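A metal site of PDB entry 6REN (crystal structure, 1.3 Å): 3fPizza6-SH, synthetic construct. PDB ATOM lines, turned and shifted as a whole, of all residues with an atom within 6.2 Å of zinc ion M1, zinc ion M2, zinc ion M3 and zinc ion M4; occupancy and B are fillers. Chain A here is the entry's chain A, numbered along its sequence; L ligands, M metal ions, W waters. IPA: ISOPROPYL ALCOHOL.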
ATOM      1  N   SER A  20      -8.096  12.850 -29.014  1.00  0.00           N
ATOM      2  CA  SER A  20      -8.028  11.834 -27.978  1.00  0.00           C
ATOM      3  C   SER A  20      -8.333  12.412 -26.605  1.00  0.00           C
ATOM      4  O   SER A  20      -9.452  12.291 -26.121  1.00  0.00           O
ATOM      5  CB  SER A  20      -6.672  11.103 -28.019  1.00  0.00           C
ATOM      6  OG  SER A  20      -5.573  11.987 -27.801  1.00  0.00           O
ATOM      7  N   GLY A  21      -7.388  13.065 -25.985  1.00  0.00           N
ATOM      8  CA  GLY A  21      -7.654  13.644 -24.690  1.00  0.00           C
ATOM      9  C   GLY A  21      -8.506  14.908 -24.766  1.00  0.00           C
ATOM     10  O   GLY A  21      -8.440  15.683 -25.731  1.00  0.00           O
ATOM     11  N   HIS A  35      -4.300  14.154 -31.551  1.00  0.00           N
ATOM     12  CA  HIS A  35      -3.268  13.109 -31.424  1.00  0.00           C
ATOM     13  C   HIS A  35      -2.495  12.913 -32.715  1.00  0.00           C
ATOM     14  O   HIS A  35      -1.256  12.796 -32.689  1.00  0.00           O
ATOM     15  CB  HIS A  35      -4.009  11.829 -31.028  1.00  0.00           C
ATOM     16  CG  HIS A  35      -3.217  10.652 -30.550  1.00  0.00           C
ATOM     17  ND1 HIS A  35      -2.708   9.673 -31.390  1.00  0.00           N
ATOM     18  CD2 HIS A  35      -3.045  10.172 -29.291  1.00  0.00           C
ATOM     19  CE1 HIS A  35      -2.173   8.704 -30.665  1.00  0.00           C
ATOM     20  NE2 HIS A  35      -2.373   8.972 -29.374  1.00  0.00           N
ATOM     21  N   THR A  60       2.435  12.007 -30.862  1.00  0.00           N
ATOM     22  CA  THR A  60       1.236  11.368 -30.332  1.00  0.00           C
ATOM     23  C   THR A  60       0.898  11.825 -28.905  1.00  0.00           C
ATOM     24  O   THR A  60       0.843  11.023 -27.969  1.00  0.00           O
ATOM     25  CB  THR A  60       1.202   9.849 -30.445  1.00  0.00           C
ATOM     26  OG1 THR A  60       2.358   9.245 -29.869  1.00  0.00           O
ATOM     27  CG2 THR A  60       1.152   9.463 -31.936  1.00  0.00           C
ATOM     28  N   PRO A  61       0.676  13.124 -28.705  1.00  0.00           N
ATOM     29  CA  PRO A  61       0.167  13.596 -27.402  1.00  0.00           C
ATOM     30  C   PRO A  61      -1.200  13.002 -27.140  1.00  0.00           C
ATOM     31  O   PRO A  61      -2.009  12.805 -28.045  1.00  0.00           O
ATOM     32  CB  PRO A  61       0.093  15.118 -27.582  1.00  0.00           C
ATOM     33  CG  PRO A  61      -0.156  15.282 -29.064  1.00  0.00           C
ATOM     34  CD  PRO A  61       0.624  14.182 -29.746  1.00  0.00           C
ATOM     35  N   HIS A  62      -1.491  12.740 -25.868  1.00  0.00           N
ATOM     36  CA  HIS A  62      -2.661  11.913 -25.564  1.00  0.00           C
ATOM     37  C   HIS A  62      -3.471  12.549 -24.427  1.00  0.00           C
ATOM     38  O   HIS A  62      -4.412  13.284 -24.666  1.00  0.00           O
ATOM     39  CB  HIS A  62      -2.194  10.483 -25.323  1.00  0.00           C
ATOM     40  CG  HIS A  62      -3.312   9.483 -25.301  1.00  0.00           C
ATOM     41  ND1 HIS A  62      -3.376   8.425 -26.187  1.00  0.00           N
ATOM     42  CD2 HIS A  62      -4.402   9.407 -24.507  1.00  0.00           C
ATOM     43  CE1 HIS A  62      -4.477   7.712 -25.916  1.00  0.00           C
ATOM     44  NE2 HIS A  62      -5.113   8.307 -24.911  1.00  0.00           N
ATOM     45  N   GLY A  63      -3.106  12.373 -23.178  1.00  0.00           N
ATOM     46  CA  GLY A  63      -3.895  12.981 -22.115  1.00  0.00           C
ATOM     47  C   GLY A  63      -3.608  14.473 -21.995  1.00  0.00           C
ATOM     48  O   GLY A  63      -2.499  14.953 -22.308  1.00  0.00           O
ATOM     49  N   HIS A  77       3.303  10.809 -25.346  1.00  0.00           N
ATOM     50  CA  HIS A  77       3.747   9.421 -25.125  1.00  0.00           C
ATOM     51  C   HIS A  77       4.798   8.940 -26.096  1.00  0.00           C
ATOM     52  O   HIS A  77       5.601   8.096 -25.707  1.00  0.00           O
ATOM     53  CB  HIS A  77       2.682   8.362 -24.838  1.00  0.00           C
ATOM     54  CG  HIS A  77       1.686   8.117 -25.927  1.00  0.00           C
ATOM     55  ND1 HIS A  77       2.008   7.544 -27.147  1.00  0.00           N
ATOM     56  CD2 HIS A  77       0.348   8.290 -25.943  1.00  0.00           C
ATOM     57  CE1 HIS A  77       0.905   7.387 -27.855  1.00  0.00           C
ATOM     58  NE2 HIS A  77      -0.121   7.822 -27.149  1.00  0.00           N
ATOM     59  N   SER A 104      -0.159   7.799 -20.770  1.00  0.00           N
ATOM     60  CA  SER A 104      -1.401   8.080 -21.495  1.00  0.00           C
ATOM     61  C   SER A 104      -2.233   9.167 -20.876  1.00  0.00           C
ATOM     62  O   SER A 104      -2.852   9.930 -21.611  1.00  0.00           O
ATOM     63  CB  SER A 104      -2.201   6.779 -21.700  1.00  0.00           C
ATOM     64  OG  SER A 104      -2.347   6.143 -20.451  1.00  0.00           O
ATOM     65  N   HIS A 119       1.159   3.988 -18.584  1.00  0.00           N
ATOM     66  CA  HIS A 119       0.390   2.904 -19.202  1.00  0.00           C
ATOM     67  C   HIS A 119       1.253   1.650 -19.420  1.00  0.00           C
ATOM     68  O   HIS A 119       0.854   0.520 -19.059  1.00  0.00           O
ATOM     69  CB  HIS A 119      -0.117   3.519 -20.526  1.00  0.00           C
ATOM     70  CG  HIS A 119      -1.114   2.726 -21.320  1.00  0.00           C
ATOM     71  ND1 HIS A 119      -0.771   1.711 -22.179  1.00  0.00           N
ATOM     72  CD2 HIS A 119      -2.424   2.994 -21.541  1.00  0.00           C
ATOM     73  CE1 HIS A 119      -1.847   1.334 -22.858  1.00  0.00           C
ATOM     74  NE2 HIS A 119      -2.873   2.084 -22.478  1.00  0.00           N
ATOM     75  N   THR A 144      -2.031  -1.976 -17.831  1.00  0.00           N
ATOM     76  CA  THR A 144      -2.214  -0.863 -18.760  1.00  0.00           C
ATOM     77  C   THR A 144      -3.257   0.155 -18.279  1.00  0.00           C
ATOM     78  O   THR A 144      -4.274   0.379 -18.947  1.00  0.00           O
ATOM     79  CB  THR A 144      -2.464  -1.278 -20.214  1.00  0.00           C
ATOM     80  OG1 THR A 144      -3.712  -1.952 -20.314  1.00  0.00           O
ATOM     81  CG2 THR A 144      -1.372  -2.161 -20.753  1.00  0.00           C
ATOM     82  N   PRO A 145      -3.024   0.772 -17.131  1.00  0.00           N
ATOM     83  CA  PRO A 145      -3.900   1.875 -16.694  1.00  0.00           C
ATOM     84  C   PRO A 145      -3.803   3.039 -17.693  1.00  0.00           C
ATOM     85  O   PRO A 145      -2.712   3.400 -18.142  1.00  0.00           O
ATOM     86  CB  PRO A 145      -3.320   2.257 -15.324  1.00  0.00           C
ATOM     87  CG  PRO A 145      -1.814   1.916 -15.465  1.00  0.00           C
ATOM     88  CD  PRO A 145      -1.799   0.645 -16.306  1.00  0.00           C
ATOM     89  N   HIS A 146      -4.953   3.612 -18.025  1.00  0.00           N
ATOM     90  CA  HIS A 146      -5.062   4.453 -19.217  1.00  0.00           C
ATOM     91  C   HIS A 146      -5.505   5.869 -18.877  1.00  0.00           C
ATOM     92  O   HIS A 146      -4.704   6.814 -19.035  1.00  0.00           O
ATOM     93  CB  HIS A 146      -5.985   3.747 -20.225  1.00  0.00           C
ATOM     94  CG  HIS A 146      -6.120   4.469 -21.542  1.00  0.00           C
ATOM     95  ND1 HIS A 146      -5.617   3.989 -22.730  1.00  0.00           N
ATOM     96  CD2 HIS A 146      -6.674   5.687 -21.820  1.00  0.00           C
ATOM     97  CE1 HIS A 146      -5.871   4.861 -23.684  1.00  0.00           C
ATOM     98  NE2 HIS A 146      -6.507   5.908 -23.177  1.00  0.00           N
ATOM     99  N   GLY A 147      -6.744   6.059 -18.433  1.00  0.00           N
ATOM    100  CA  GLY A 147      -7.270   7.362 -18.072  1.00  0.00           C
ATOM    101  C   GLY A 147      -7.105   7.579 -16.579  1.00  0.00           C
ATOM    102  O   GLY A 147      -7.123   6.622 -15.798  1.00  0.00           O
ATOM    103  N   HIS A 161      -7.619  -0.730 -17.937  1.00  0.00           N
ATOM    104  CA  HIS A 161      -8.335  -1.477 -18.974  1.00  0.00           C
ATOM    105  C   HIS A 161      -7.750  -2.852 -19.251  1.00  0.00           C
ATOM    106  O   HIS A 161      -8.476  -3.682 -19.792  1.00  0.00           O
ATOM    107  CB  HIS A 161      -8.650  -0.651 -20.246  1.00  0.00           C
ATOM    108  CG  HIS A 161      -7.452  -0.327 -21.122  1.00  0.00           C
ATOM    109  ND1 HIS A 161      -6.659  -1.272 -21.754  1.00  0.00           N
ATOM    110  CD2 HIS A 161      -6.998   0.875 -21.547  1.00  0.00           C
ATOM    111  CE1 HIS A 161      -5.727  -0.653 -22.479  1.00  0.00           C
ATOM    112  NE2 HIS A 161      -5.910   0.660 -22.374  1.00  0.00           N
ATOM    113  N   PRO A 187     -12.328   0.275 -21.040  1.00  0.00           N
ATOM    114  CA  PRO A 187     -12.560   1.715 -20.827  1.00  0.00           C
ATOM    115  C   PRO A 187     -11.321   2.570 -21.091  1.00  0.00           C
ATOM    116  O   PRO A 187     -10.185   2.145 -20.833  1.00  0.00           O
ATOM    117  CB  PRO A 187     -12.974   1.789 -19.359  1.00  0.00           C
ATOM    118  CG  PRO A 187     -12.314   0.603 -18.724  1.00  0.00           C
ATOM    119  CD  PRO A 187     -12.385  -0.489 -19.773  1.00  0.00           C
ATOM    120  N   SER A 188     -11.570   3.791 -21.594  1.00  0.00           N
ATOM    121  CA  SER A 188     -10.482   4.745 -21.909  1.00  0.00           C
ATOM    122  C   SER A 188     -10.591   5.986 -21.018  1.00  0.00           C
ATOM    123  O   SER A 188      -9.987   6.032 -19.945  1.00  0.00           O
ATOM    124  CB  SER A 188     -10.463   5.073 -23.416  1.00  0.00           C
ATOM    125  OG  SER A 188     -11.774   5.450 -23.885  1.00  0.00           O
ATOM    126  N   GLY A 189     -11.290   7.035 -21.420  1.00  0.00           N
ATOM    127  CA  GLY A 189     -11.345   8.235 -20.594  1.00  0.00           C
ATOM    128  C   GLY A 189     -12.152   8.028 -19.327  1.00  0.00           C
ATOM    129  O   GLY A 189     -13.113   7.247 -19.272  1.00  0.00           O
ATOM    130  N   HIS A 203     -14.983   2.313 -24.306  1.00  0.00           N
ATOM    131  CA  HIS A 203     -14.503   2.450 -25.679  1.00  0.00           C
ATOM    132  C   HIS A 203     -14.947   1.299 -26.561  1.00  0.00           C
ATOM    133  O   HIS A 203     -15.328   1.502 -27.713  1.00  0.00           O
ATOM    134  CB  HIS A 203     -12.967   2.553 -25.633  1.00  0.00           C
ATOM    135  CG  HIS A 203     -12.317   3.084 -26.879  1.00  0.00           C
ATOM    136  ND1 HIS A 203     -12.306   2.426 -28.102  1.00  0.00           N
ATOM    137  CD2 HIS A 203     -11.588   4.213 -27.058  1.00  0.00           C
ATOM    138  CE1 HIS A 203     -11.600   3.145 -28.977  1.00  0.00           C
ATOM    139  NE2 HIS A 203     -11.118   4.214 -28.359  1.00  0.00           N
ATOM    140  N   THR A 228     -16.603   6.582 -32.614  1.00  0.00           N
ATOM    141  CA  THR A 228     -15.571   5.967 -31.764  1.00  0.00           C
ATOM    142  C   THR A 228     -15.176   6.959 -30.667  1.00  0.00           C
ATOM    143  O   THR A 228     -14.123   7.614 -30.739  1.00  0.00           O
ATOM    144  CB  THR A 228     -14.370   5.491 -32.602  1.00  0.00           C
ATOM    145  OG1 THR A 228     -14.849   4.682 -33.691  1.00  0.00           O
ATOM    146  CG2 THR A 228     -13.401   4.650 -31.788  1.00  0.00           C
ATOM    147  N   PRO A 229     -15.997   7.123 -29.647  1.00  0.00           N
ATOM    148  CA  PRO A 229     -15.647   8.038 -28.543  1.00  0.00           C
ATOM    149  C   PRO A 229     -14.429   7.537 -27.776  1.00  0.00           C
ATOM    150  O   PRO A 229     -14.141   6.328 -27.709  1.00  0.00           O
ATOM    151  CB  PRO A 229     -16.907   8.017 -27.669  1.00  0.00           C
ATOM    152  CG  PRO A 229     -17.547   6.661 -27.943  1.00  0.00           C
ATOM    153  CD  PRO A 229     -17.311   6.473 -29.433  1.00  0.00           C
ATOM    154  N   HIS A 230     -13.687   8.487 -27.174  1.00  0.00           N
ATOM    155  CA  HIS A 230     -12.426   8.144 -26.535  1.00  0.00           C
ATOM    156  C   HIS A 230     -12.237   8.865 -25.208  1.00  0.00           C
ATOM    157  O   HIS A 230     -12.180   8.230 -24.140  1.00  0.00           O
ATOM    158  CB  HIS A 230     -11.238   8.355 -27.493  1.00  0.00           C
ATOM    159  CG  HIS A 230      -9.956   7.857 -26.912  1.00  0.00           C
ATOM    160  ND1 HIS A 230      -9.303   6.725 -27.331  1.00  0.00           N
ATOM    161  CD2 HIS A 230      -9.232   8.349 -25.871  1.00  0.00           C
ATOM    162  CE1 HIS A 230      -8.246   6.514 -26.538  1.00  0.00           C
ATOM    163  NE2 HIS A 230      -8.176   7.487 -25.630  1.00  0.00           N
ATOM    164  N   GLY A 231     -12.081  10.181 -25.245  1.00  0.00           N
ATOM    165  CA  GLY A 231     -11.862  10.953 -24.032  1.00  0.00           C
ATOM    166  C   GLY A 231     -13.156  11.552 -23.518  1.00  0.00           C
ATOM    167  O   GLY A 231     -14.112  11.784 -24.291  1.00  0.00           O
ATOM    168  N   HIS A 245     -12.830  10.010 -32.244  1.00  0.00           N
ATOM    169  CA  HIS A 245     -11.844   9.883 -33.321  1.00  0.00           C
ATOM    170  C   HIS A 245     -12.326   9.018 -34.469  1.00  0.00           C
ATOM    171  O   HIS A 245     -11.582   8.840 -35.443  1.00  0.00           O
ATOM    172  CB  HIS A 245     -10.437   9.492 -32.827  1.00  0.00           C
ATOM    173  CG  HIS A 245     -10.337   8.183 -32.081  1.00  0.00           C
ATOM    174  ND1 HIS A 245     -10.492   6.959 -32.686  1.00  0.00           N
ATOM    175  CD2 HIS A 245     -10.054   7.929 -30.782  1.00  0.00           C
ATOM    176  CE1 HIS A 245     -10.336   6.009 -31.787  1.00  0.00           C
ATOM    177  NE2 HIS A 245     -10.061   6.562 -30.612  1.00  0.00           N
HETATM  178  C1  IPA L   1      -3.860   0.057 -24.890  1.00  0.00           C
HETATM  179  C2  IPA L   1      -4.279   1.141 -25.738  1.00  0.00           C
HETATM  180  C3  IPA L   1      -4.337   0.910 -27.234  1.00  0.00           C
HETATM  181  O2  IPA L   1      -4.840   2.208 -25.180  1.00  0.00           O
HETATM  182  C1  IPA L   2      -8.926   3.426 -30.704  1.00  0.00           C
HETATM  183  C2  IPA L   2      -7.806   3.404 -29.736  1.00  0.00           C
HETATM  184  C3  IPA L   2      -6.447   2.910 -30.186  1.00  0.00           C
HETATM  185  O2  IPA L   2      -7.933   4.512 -28.981  1.00  0.00           O
HETATM  186  C1  IPA L   3      -2.596   3.974 -29.507  1.00  0.00           C
HETATM  187  C2  IPA L   3      -2.277   5.458 -29.424  1.00  0.00           C
HETATM  188  C3  IPA L   3      -0.857   5.722 -29.895  1.00  0.00           C
HETATM  189  O2  IPA L   3      -2.597   6.038 -28.174  1.00  0.00           O
HETATM  190 ZN    ZN M   1      -4.801   2.157 -23.179  1.00  0.00          ZN
HETATM  191 ZN    ZN M   2      -6.876   7.643 -24.142  1.00  0.00          ZN
HETATM  192 ZN    ZN M   3      -9.663   5.490 -28.926  1.00  0.00          ZN
HETATM  193 ZN    ZN M   4      -2.079   7.865 -27.673  1.00  0.00          ZN
HETATM  194  O   HOH W   1      -8.028   9.088 -22.698  1.00  0.00           O
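Of the 24 residues printed, 3 come within 4 Å of zinc ion M2.
Three residues have an atom within 4 Å of zinc ion M1: His 119, His 146 and His 161. The nearest printed residue that does not touch zinc ion M1 is Thr 144 (4.6 Å).
The nearest printed residue that does not touch zinc ion M3 is Pro 229 (4.7 Å).
O of His 230 is in hydrogen-bond range of OG of Ser 188. O of His 230 lies within hydrogen-bond range of N of Gly 189 (3.1 Å). The backbone carbonyl oxygen of His 146 lies within hydrogen-bond range of the side-chain hydroxyl of Ser 104 (2.8 Å). A ring nitrogen (ND1) of His 77 lies close to the side-chain hydroxyl (OG1) of Thr 60, 3.2 Å away. The side-chain hydroxyl (OG1) of Thr 144 sits close to a ring nitrogen (ND1) of His 161, 3.3 Å away. The backbone NH (N) of Gly 21 sits close to the backbone carbonyl oxygen (O) of His 62, 3.3 Å away. O of Thr 228 sits at hydrogen-bond distance from N of His 245.
An oxygen (O2) of IPA L2 is bound to zinc ion M3 (2.0 Å). NE2 of His 203 is bound to zinc ion M3 (2.0 Å). A ring nitrogen (NE2) of His 245 binds zinc ion M3 (2.0 Å). A ring nitrogen (ND1) of His 230 binds zinc ion M3 (2.0 Å). Zinc ion M3 has four donor atoms within binding distance.
Zinc ion M2 is bound by a ring nitrogen (NE2) of His 230 (2.0 Å), a ring nitrogen (NE2) of His 146 (2.0 Å), a ring nitrogen (NE2) of His 62 (2.0 Å) and water W1 (2.3 Å).
Zinc ion M4 is bound by O2 of IPA L3 (2.0 Å). Zinc ion M4 is bound by a ring nitrogen (NE2) of His 77 (2.0 Å). ND1 of His 62 is bound to zinc ion M4. Zinc ion M4 is bound by NE2 of His 35, 2.1 Å away.
Along chain A the residues within 4 Å of zinc ion M4 span positions 35 to 77.
Zinc ion M1 is bound by an oxygen (O2) of IPA L1 (2.0 Å), a ring nitrogen (NE2) of His 161 (2.0 Å), a ring nitrogen (NE2) of His 119 (2.1 Å) and a ring nitrogen (ND1) of His 146 (2.1 Å).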
